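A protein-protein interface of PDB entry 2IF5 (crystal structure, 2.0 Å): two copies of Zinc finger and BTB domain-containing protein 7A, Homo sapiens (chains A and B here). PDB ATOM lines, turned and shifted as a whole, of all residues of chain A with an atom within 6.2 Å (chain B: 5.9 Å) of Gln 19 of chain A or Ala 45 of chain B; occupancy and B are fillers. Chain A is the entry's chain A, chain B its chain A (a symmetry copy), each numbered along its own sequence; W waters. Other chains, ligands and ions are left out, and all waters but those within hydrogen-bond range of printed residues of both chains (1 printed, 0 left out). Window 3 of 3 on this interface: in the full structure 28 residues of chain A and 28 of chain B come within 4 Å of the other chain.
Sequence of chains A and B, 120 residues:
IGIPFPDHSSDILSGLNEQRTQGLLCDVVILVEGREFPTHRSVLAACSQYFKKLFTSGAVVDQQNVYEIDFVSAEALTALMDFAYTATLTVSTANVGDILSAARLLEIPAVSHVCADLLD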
ATOM      1  N   SER A  14     -23.802  -0.800 -13.862  1.00  0.00           N
ATOM      2  CA  SER A  14     -23.170  -2.074 -13.691  1.00  0.00           C
ATOM      3  C   SER A  14     -23.041  -2.847 -15.005  1.00  0.00           C
ATOM      4  O   SER A  14     -22.033  -3.521 -15.257  1.00  0.00           O
ATOM      5  CB  SER A  14     -24.013  -2.895 -12.702  1.00  0.00           C
ATOM      6  OG  SER A  14     -23.265  -4.003 -12.283  1.00  0.00           O
ATOM      7  N   GLY A  15     -24.101  -2.831 -15.807  1.00  0.00           N
ATOM      8  CA  GLY A  15     -24.104  -3.495 -17.078  1.00  0.00           C
ATOM      9  C   GLY A  15     -23.119  -2.866 -18.019  1.00  0.00           C
ATOM     10  O   GLY A  15     -22.409  -3.567 -18.716  1.00  0.00           O
ATOM     11  N   LEU A  16     -23.007  -1.536 -17.995  1.00  0.00           N
ATOM     12  CA  LEU A  16     -22.062  -0.843 -18.869  1.00  0.00           C
ATOM     13  C   LEU A  16     -20.636  -1.148 -18.405  1.00  0.00           C
ATOM     14  O   LEU A  16     -19.736  -1.340 -19.232  1.00  0.00           O
ATOM     15  CB  LEU A  16     -22.340   0.686 -18.901  1.00  0.00           C
ATOM     16  CG  LEU A  16     -23.704   1.083 -19.458  1.00  0.00           C
ATOM     17  CD1 LEU A  16     -24.062   2.558 -19.143  1.00  0.00           C
ATOM     18  CD2 LEU A  16     -23.692   0.875 -20.963  1.00  0.00           C
ATOM     19  N   ASN A  17     -20.443  -1.202 -17.087  1.00  0.00           N
ATOM     20  CA  ASN A  17     -19.146  -1.601 -16.525  1.00  0.00           C
ATOM     21  C   ASN A  17     -18.772  -3.055 -16.913  1.00  0.00           C
ATOM     22  O   ASN A  17     -17.630  -3.329 -17.217  1.00  0.00           O
ATOM     23  CB  ASN A  17     -19.159  -1.452 -15.009  1.00  0.00           C
ATOM     24  CG  ASN A  17     -17.769  -1.525 -14.400  1.00  0.00           C
ATOM     25  OD1 ASN A  17     -17.568  -2.139 -13.350  1.00  0.00           O
ATOM     26  ND2 ASN A  17     -16.816  -0.934 -15.071  1.00  0.00           N
ATOM     27  N   GLU A  18     -19.727  -3.974 -16.889  1.00  0.00           N
ATOM     28  CA  GLU A  18     -19.519  -5.347 -17.411  1.00  0.00           C
ATOM     29  C   GLU A  18     -19.004  -5.357 -18.868  1.00  0.00           C
ATOM     30  O   GLU A  18     -18.014  -6.027 -19.201  1.00  0.00           O
ATOM     31  CB  GLU A  18     -20.837  -6.136 -17.347  1.00  0.00           C
ATOM     32  CG  GLU A  18     -21.115  -6.793 -16.016  1.00  0.00           C
ATOM     33  CD  GLU A  18     -22.489  -7.436 -15.942  1.00  0.00           C
ATOM     34  OE1 GLU A  18     -23.091  -7.750 -16.999  1.00  0.00           O
ATOM     35  OE2 GLU A  18     -22.965  -7.643 -14.804  1.00  0.00           O
ATOM     36  N   GLN A  19     -19.711  -4.628 -19.735  1.00  0.00           N
ATOM     37  CA  GLN A  19     -19.283  -4.383 -21.120  1.00  0.00           C
ATOM     38  C   GLN A  19     -17.859  -3.891 -21.225  1.00  0.00           C
ATOM     39  O   GLN A  19     -17.073  -4.428 -22.035  1.00  0.00           O
ATOM     40  CB  GLN A  19     -20.238  -3.422 -21.832  1.00  0.00           C
ATOM     41  CG  GLN A  19     -21.631  -4.079 -22.140  1.00  0.00           C
ATOM     42  CD  GLN A  19     -22.697  -3.074 -22.559  1.00  0.00           C
ATOM     43  OE1 GLN A  19     -23.899  -3.231 -22.262  1.00  0.00           O
ATOM     44  NE2 GLN A  19     -22.275  -2.047 -23.260  1.00  0.00           N
ATOM     45  N   ARG A  20     -17.531  -2.852 -20.446  1.00  0.00           N
ATOM     46  CA  ARG A  20     -16.171  -2.331 -20.377  1.00  0.00           C
ATOM     47  C   ARG A  20     -15.176  -3.399 -19.890  1.00  0.00           C
ATOM     48  O   ARG A  20     -14.158  -3.617 -20.543  1.00  0.00           O
ATOM     49  CB  ARG A  20     -16.113  -1.083 -19.489  1.00  0.00           C
ATOM     50  CG  ARG A  20     -14.758  -0.410 -19.459  1.00  0.00           C
ATOM     51  CD  ARG A  20     -14.740   0.738 -18.472  1.00  0.00           C
ATOM     52  NE  ARG A  20     -14.906   0.365 -17.067  1.00  0.00           N
ATOM     53  CZ  ARG A  20     -14.045   0.706 -16.108  1.00  0.00           C
ATOM     54  NH1 ARG A  20     -12.955   1.375 -16.440  1.00  0.00           N
ATOM     55  NH2 ARG A  20     -14.248   0.343 -14.836  1.00  0.00           N
ATOM     56  N   THR A  21     -15.469  -4.045 -18.756  1.00  0.00           N
ATOM     57  CA  THR A  21     -14.629  -5.129 -18.216  1.00  0.00           C
ATOM     58  C   THR A  21     -14.364  -6.185 -19.295  1.00  0.00           C
ATOM     59  O   THR A  21     -13.212  -6.526 -19.564  1.00  0.00           O
ATOM     60  CB  THR A  21     -15.273  -5.791 -16.942  1.00  0.00           C
ATOM     61  OG1 THR A  21     -15.164  -4.892 -15.838  1.00  0.00           O
ATOM     62  CG2 THR A  21     -14.581  -7.103 -16.567  1.00  0.00           C
ATOM     63  N   GLN A  22     -15.427  -6.643 -19.949  1.00  0.00           N
ATOM     64  CA  GLN A  22     -15.359  -7.708 -20.962  1.00  0.00           C
ATOM     65  C   GLN A  22     -14.959  -7.287 -22.382  1.00  0.00           C
ATOM     66  O   GLN A  22     -14.890  -8.133 -23.293  1.00  0.00           O
ATOM     67  CB  GLN A  22     -16.689  -8.451 -21.000  1.00  0.00           C
ATOM     68  CG  GLN A  22     -16.870  -9.355 -19.800  1.00  0.00           C
ATOM     69  CD  GLN A  22     -18.276  -9.369 -19.278  1.00  0.00           C
ATOM     70  OE1 GLN A  22     -19.218  -9.787 -19.968  1.00  0.00           O
ATOM     71  NE2 GLN A  22     -18.438  -8.914 -18.039  1.00  0.00           N
ATOM     72  N   GLY A  23     -14.706  -5.997 -22.574  1.00  0.00           N
ATOM     73  CA  GLY A  23     -14.425  -5.459 -23.899  1.00  0.00           C
ATOM     74  C   GLY A  23     -15.551  -5.666 -24.892  1.00  0.00           C
ATOM     75  O   GLY A  23     -15.311  -5.925 -26.063  1.00  0.00           O
ATOM     76  N   LEU A  24     -16.784  -5.532 -24.427  1.00  0.00           N
ATOM     77  CA  LEU A  24     -17.968  -5.706 -25.278  1.00  0.00           C
ATOM     78  C   LEU A  24     -18.684  -4.377 -25.546  1.00  0.00           C
ATOM     79  O   LEU A  24     -18.823  -3.527 -24.634  1.00  0.00           O
ATOM     80  CB  LEU A  24     -18.932  -6.714 -24.653  1.00  0.00           C
ATOM     81  CG  LEU A  24     -18.611  -8.210 -24.578  1.00  0.00           C
ATOM     82  CD1 LEU A  24     -19.572  -8.886 -23.611  1.00  0.00           C
ATOM     83  CD2 LEU A  24     -18.671  -8.894 -25.960  1.00  0.00           C
ATOM     84  N   LEU A  25     -19.091  -4.175 -26.802  1.00  0.00           N
ATOM     85  CA  LEU A  25     -19.868  -2.993 -27.215  1.00  0.00           C
ATOM     86  C   LEU A  25     -19.194  -1.646 -26.902  1.00  0.00           C
ATOM     87  O   LEU A  25     -19.859  -0.635 -26.813  1.00  0.00           O
ATOM     88  CB  LEU A  25     -21.311  -3.028 -26.636  1.00  0.00           C
ATOM     89  CG  LEU A  25     -22.141  -4.288 -26.889  1.00  0.00           C
ATOM     90  CD1 LEU A  25     -23.477  -4.237 -26.146  1.00  0.00           C
ATOM     91  CD2 LEU A  25     -22.384  -4.480 -28.397  1.00  0.00           C
ATOM     92  N   CYS A  26     -17.869  -1.654 -26.796  1.00  0.00           N
ATOM     93  CA  CYS A  26     -17.077  -0.453 -26.623  1.00  0.00           C
ATOM     94  C   CYS A  26     -16.797   0.107 -28.003  1.00  0.00           C
ATOM     95  O   CYS A  26     -16.405  -0.639 -28.881  1.00  0.00           O
ATOM     96  CB  CYS A  26     -15.775  -0.825 -25.931  1.00  0.00           C
ATOM     97  SG  CYS A  26     -16.076  -1.359 -24.229  1.00  0.00           S
ATOM     98  N   HIS A  40     -17.076   3.420 -23.870  1.00  0.00           N
ATOM     99  CA  HIS A  40     -18.227   3.882 -24.647  1.00  0.00           C
ATOM    100  C   HIS A  40     -18.154   5.375 -24.744  1.00  0.00           C
ATOM    101  O   HIS A  40     -17.978   6.047 -23.714  1.00  0.00           O
ATOM    102  CB  HIS A  40     -19.557   3.524 -23.947  1.00  0.00           C
ATOM    103  CG  HIS A  40     -19.613   2.118 -23.436  1.00  0.00           C
ATOM    104  ND1 HIS A  40     -20.302   1.109 -24.081  1.00  0.00           N
ATOM    105  CD2 HIS A  40     -19.062   1.550 -22.341  1.00  0.00           C
ATOM    106  CE1 HIS A  40     -20.175  -0.018 -23.402  1.00  0.00           C
ATOM    107  NE2 HIS A  40     -19.418   0.221 -22.348  1.00  0.00           N
ATOM    108  N   HIS B  40     -28.912   3.637 -27.947  1.00  0.00           N
ATOM    109  CA  HIS B  40     -27.560   3.110 -27.757  1.00  0.00           C
ATOM    110  C   HIS B  40     -27.659   1.625 -27.583  1.00  0.00           C
ATOM    111  O   HIS B  40     -28.468   1.157 -26.765  1.00  0.00           O
ATOM    112  CB  HIS B  40     -26.906   3.686 -26.481  1.00  0.00           C
ATOM    113  CG  HIS B  40     -27.078   5.165 -26.329  1.00  0.00           C
ATOM    114  ND1 HIS B  40     -26.073   6.073 -26.606  1.00  0.00           N
ATOM    115  CD2 HIS B  40     -28.139   5.898 -25.931  1.00  0.00           C
ATOM    116  CE1 HIS B  40     -26.509   7.300 -26.381  1.00  0.00           C
ATOM    117  NE2 HIS B  40     -27.764   7.222 -25.980  1.00  0.00           N
ATOM    118  N   ARG B  41     -26.843   0.886 -28.344  1.00  0.00           N
ATOM    119  CA  ARG B  41     -26.723  -0.567 -28.210  1.00  0.00           C
ATOM    120  C   ARG B  41     -26.410  -0.952 -26.786  1.00  0.00           C
ATOM    121  O   ARG B  41     -26.944  -1.915 -26.251  1.00  0.00           O
ATOM    122  CB  ARG B  41     -25.555  -1.087 -29.059  1.00  0.00           C
ATOM    123  CG  ARG B  41     -25.894  -1.416 -30.521  1.00  0.00           C
ATOM    124  CD  ARG B  41     -24.609  -1.529 -31.378  1.00  0.00           C
ATOM    125  NE  ARG B  41     -24.909  -1.116 -32.748  1.00  0.00           N
ATOM    126  CZ  ARG B  41     -25.253  -1.930 -33.741  1.00  0.00           C
ATOM    127  NH1 ARG B  41     -25.277  -3.251 -33.574  1.00  0.00           N
ATOM    128  NH2 ARG B  41     -25.560  -1.413 -34.925  1.00  0.00           N
ATOM    129  N   SER B  42     -25.438  -0.236 -26.216  1.00  0.00           N
ATOM    130  CA  SER B  42     -24.922  -0.508 -24.896  1.00  0.00           C
ATOM    131  C   SER B  42     -25.984  -0.387 -23.818  1.00  0.00           C
ATOM    132  O   SER B  42     -26.053  -1.250 -22.964  1.00  0.00           O
ATOM    133  CB  SER B  42     -23.741   0.437 -24.590  1.00  0.00           C
ATOM    134  OG  SER B  42     -24.220   1.758 -24.588  1.00  0.00           O
ATOM    135  N   VAL B  43     -26.782   0.672 -23.849  1.00  0.00           N
ATOM    136  CA  VAL B  43     -27.887   0.859 -22.875  1.00  0.00           C
ATOM    137  C   VAL B  43     -28.935  -0.249 -23.019  1.00  0.00           C
ATOM    138  O   VAL B  43     -29.338  -0.886 -22.029  1.00  0.00           O
ATOM    139  CB  VAL B  43     -28.552   2.270 -22.978  1.00  0.00           C
ATOM    140  CG1 VAL B  43     -29.713   2.385 -21.998  1.00  0.00           C
ATOM    141  CG2 VAL B  43     -27.541   3.375 -22.663  1.00  0.00           C
ATOM    142  N   LEU B  44     -29.358  -0.512 -24.256  1.00  0.00           N
ATOM    143  CA  LEU B  44     -30.283  -1.633 -24.474  1.00  0.00           C
ATOM    144  C   LEU B  44     -29.733  -2.954 -23.943  1.00  0.00           C
ATOM    145  O   LEU B  44     -30.427  -3.649 -23.211  1.00  0.00           O
ATOM    146  CB  LEU B  44     -30.718  -1.750 -25.942  1.00  0.00           C
ATOM    147  CG  LEU B  44     -31.363  -0.496 -26.532  1.00  0.00           C
ATOM    148  CD1 LEU B  44     -31.717  -0.678 -28.015  1.00  0.00           C
ATOM    149  CD2 LEU B  44     -32.587  -0.049 -25.717  1.00  0.00           C
ATOM    150  N   ALA B  45     -28.488  -3.288 -24.261  1.00  0.00           N
ATOM    151  CA  ALA B  45     -27.897  -4.529 -23.769  1.00  0.00           C
ATOM    152  C   ALA B  45     -27.740  -4.628 -22.250  1.00  0.00           C
ATOM    153  O   ALA B  45     -27.723  -5.720 -21.702  1.00  0.00           O
ATOM    154  CB  ALA B  45     -26.524  -4.798 -24.452  1.00  0.00           C
ATOM    155  N   ALA B  46     -27.576  -3.499 -21.580  1.00  0.00           N
ATOM    156  CA  ALA B  46     -27.444  -3.473 -20.114  1.00  0.00           C
ATOM    157  C   ALA B  46     -28.760  -3.769 -19.397  1.00  0.00           C
ATOM    158  O   ALA B  46     -28.768  -4.138 -18.221  1.00  0.00           O
ATOM    159  CB  ALA B  46     -26.895  -2.098 -19.669  1.00  0.00           C
ATOM    160  N   CYS B  47     -29.882  -3.607 -20.071  1.00  0.00           N
ATOM    161  CA  CYS B  47     -31.141  -3.973 -19.395  1.00  0.00           C
ATOM    162  C   CYS B  47     -32.048  -4.984 -20.039  1.00  0.00           C
ATOM    163  O   CYS B  47     -33.082  -5.314 -19.461  1.00  0.00           O
ATOM    164  CB  CYS B  47     -31.962  -2.752 -18.993  1.00  0.00           C
ATOM    165  SG  CYS B  47     -32.820  -1.928 -20.287  1.00  0.00           S
ATOM    166  N   SER B  48     -31.705  -5.428 -21.247  1.00  0.00           N
ATOM    167  CA  SER B  48     -32.543  -6.394 -21.939  1.00  0.00           C
ATOM    168  C   SER B  48     -31.630  -7.501 -22.415  1.00  0.00           C
ATOM    169  O   SER B  48     -30.667  -7.217 -23.135  1.00  0.00           O
ATOM    170  CB  SER B  48     -33.218  -5.755 -23.156  1.00  0.00           C
ATOM    171  OG  SER B  48     -33.678  -6.764 -24.070  1.00  0.00           O
ATOM    172  N   GLN B  49     -31.926  -8.744 -22.018  1.00  0.00           N
ATOM    173  CA  GLN B  49     -31.135  -9.875 -22.498  1.00  0.00           C
ATOM    174  C   GLN B  49     -31.412 -10.176 -23.980  1.00  0.00           C
ATOM    175  O   GLN B  49     -30.514 -10.613 -24.700  1.00  0.00           O
ATOM    176  CB  GLN B  49     -31.351 -11.123 -21.639  1.00  0.00           C
ATOM    177  CG  GLN B  49     -30.410 -12.280 -22.008  1.00  0.00           C
ATOM    178  CD  GLN B  49     -28.941 -11.990 -21.689  1.00  0.00           C
ATOM    179  OE1 GLN B  49     -28.631 -11.220 -20.768  1.00  0.00           O
ATOM    180  NE2 GLN B  49     -28.024 -12.616 -22.445  1.00  0.00           N
ATOM    181  N   PHE B  51     -31.787  -7.891 -26.230  1.00  0.00           N
ATOM    182  CA  PHE B  51     -30.896  -6.986 -26.942  1.00  0.00           C
ATOM    183  C   PHE B  51     -29.433  -7.295 -26.735  1.00  0.00           C
ATOM    184  O   PHE B  51     -28.664  -7.099 -27.655  1.00  0.00           O
ATOM    185  CB  PHE B  51     -31.168  -5.537 -26.581  1.00  0.00           C
ATOM    186  CG  PHE B  51     -32.397  -4.954 -27.248  1.00  0.00           C
ATOM    187  CD1 PHE B  51     -33.402  -4.416 -26.480  1.00  0.00           C
ATOM    188  CD2 PHE B  51     -32.513  -4.907 -28.636  1.00  0.00           C
ATOM    189  CE1 PHE B  51     -34.509  -3.835 -27.059  1.00  0.00           C
ATOM    190  CE2 PHE B  51     -33.650  -4.333 -29.247  1.00  0.00           C
ATOM    191  CZ  PHE B  51     -34.645  -3.806 -28.461  1.00  0.00           C
ATOM    192  N   LYS B  52     -29.040  -7.776 -25.555  1.00  0.00           N
ATOM    193  CA  LYS B  52     -27.625  -8.131 -25.343  1.00  0.00           C
ATOM    194  C   LYS B  52     -27.239  -9.245 -26.306  1.00  0.00           C
ATOM    195  O   LYS B  52     -26.209  -9.167 -26.969  1.00  0.00           O
ATOM    196  CB  LYS B  52     -27.323  -8.546 -23.902  1.00  0.00           C
ATOM    197  CG  LYS B  52     -25.793  -8.665 -23.612  1.00  0.00           C
ATOM    198  CD  LYS B  52     -25.458  -8.892 -22.139  1.00  0.00           C
ATOM    199  CE  LYS B  52     -24.083  -9.597 -21.958  1.00  0.00           C
ATOM    200  NZ  LYS B  52     -23.786 -10.061 -20.537  1.00  0.00           N
ATOM    201  N   PHE B  55     -27.059  -7.879 -29.963  1.00  0.00           N
ATOM    202  CA  PHE B  55     -25.922  -7.027 -30.305  1.00  0.00           C
ATOM    203  C   PHE B  55     -24.547  -7.640 -30.070  1.00  0.00           C
ATOM    204  O   PHE B  55     -23.532  -7.088 -30.539  1.00  0.00           O
ATOM    205  CB  PHE B  55     -26.010  -5.665 -29.597  1.00  0.00           C
ATOM    206  CG  PHE B  55     -27.260  -4.892 -29.935  1.00  0.00           C
ATOM    207  CD1 PHE B  55     -27.975  -4.245 -28.944  1.00  0.00           C
ATOM    208  CD2 PHE B  55     -27.713  -4.818 -31.244  1.00  0.00           C
ATOM    209  CE1 PHE B  55     -29.150  -3.525 -29.249  1.00  0.00           C
ATOM    210  CE2 PHE B  55     -28.890  -4.123 -31.566  1.00  0.00           C
ATOM    211  CZ  PHE B  55     -29.601  -3.476 -30.546  1.00  0.00           C
ATOM    212  N   THR B  56     -24.485  -8.748 -29.341  1.00  0.00           N
ATOM    213  CA  THR B  56     -23.176  -9.364 -29.089  1.00  0.00           C
ATOM    214  C   THR B  56     -22.981 -10.618 -29.937  1.00  0.00           C
ATOM    215  O   THR B  56     -22.005 -11.361 -29.769  1.00  0.00           O
ATOM    216  CB  THR B  56     -22.920  -9.637 -27.593  1.00  0.00           C
ATOM    217  OG1 THR B  56     -23.927 -10.508 -27.068  1.00  0.00           O
ATOM    218  CG2 THR B  56     -22.893  -8.338 -26.797  1.00  0.00           C
HETATM  219  O   HOH W   1     -24.640  -5.728 -20.618  1.00  0.00           O
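The side-chain amide oxygen of Gln 19 of chain A sits close to the backbone carbonyl oxygen of Ser 42 of chain B (3.0 Å).
NE2 of His 40 of chain A lies within hydrogen-bond range of O of Leu 16 of chain A, 3.5 Å away. N of Leu 24 of chain A lies within hydrogen-bond range of O of Gln 19 of chain A, 2.7 Å away. The backbone carbonyl oxygen (O) of Leu 25 of chain A lies within hydrogen-bond range of a ring nitrogen (ND1) of His 40 of chain A, 3.3 Å away.
Among the printed residues, merely in contact across the chains: Leu 16 of chain A with Ser 42 of chain B (3.7 Å), Gln 19 of chain A with Ala 45 of chain B (3.8 Å), Gln 19 of chain A with Ala 46 of chain B (3.7 Å), Leu 25 of chain A with Ala 45 of chain B (3.5 Å), Leu 25 of chain A with Phe 55 of chain B (3.6 Å) and His 40 of chain A with Ser 42 of chain B (3.5 Å).
1 position is printed for both chains. Of the 7 pairs that touch across the chains among the printed residues, none has its exchanged pair printed and touching as well.
Hydrophobic or aromatic side chains of chain B within 4 Å of the printed part of chain A: Ala 45 and Phe 55. Printed residues of chain A that touch a printed residue of chain B: Leu 16, Gln 19, Leu 25 and His 40. Hydrophobic or aromatic side chains of chain A within 4 Å of the printed part of chain B: Leu 16, Leu 25 and His 40. Among the printed residues, no Asp or Glu carboxylate lies within 4 Å of a Lys or Arg side-chain nitrogen of the other chain.
Of the printed residues of chain B, Leu 16 of chain A touches Ser 42 (3.7 Å). Gln 19 of chain A touches just these residues of chain B: Ser 42, Ala 45 and Ala 46. Printed residues of chain B within 4 Å of Leu 25 of chain A: Ala 45 (3.5 Å) and Phe 55 (3.6 Å). Of chain A, only Gln 19 and Leu 25 come within 4 Å of Ala 45 of chain B. Of the printed residues of chain A, Ala 46 of chain B touches Gln 19 (3.7 Å). The nearest printed residue of chain A that does not touch Ala 45 of chain B is Gly 15 of chain A (6.3 Å).
Water W1 bridges OE1 of Gln 19 of chain A (3.1 Å) and O of Ala 45 of chain B (3.3 Å).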
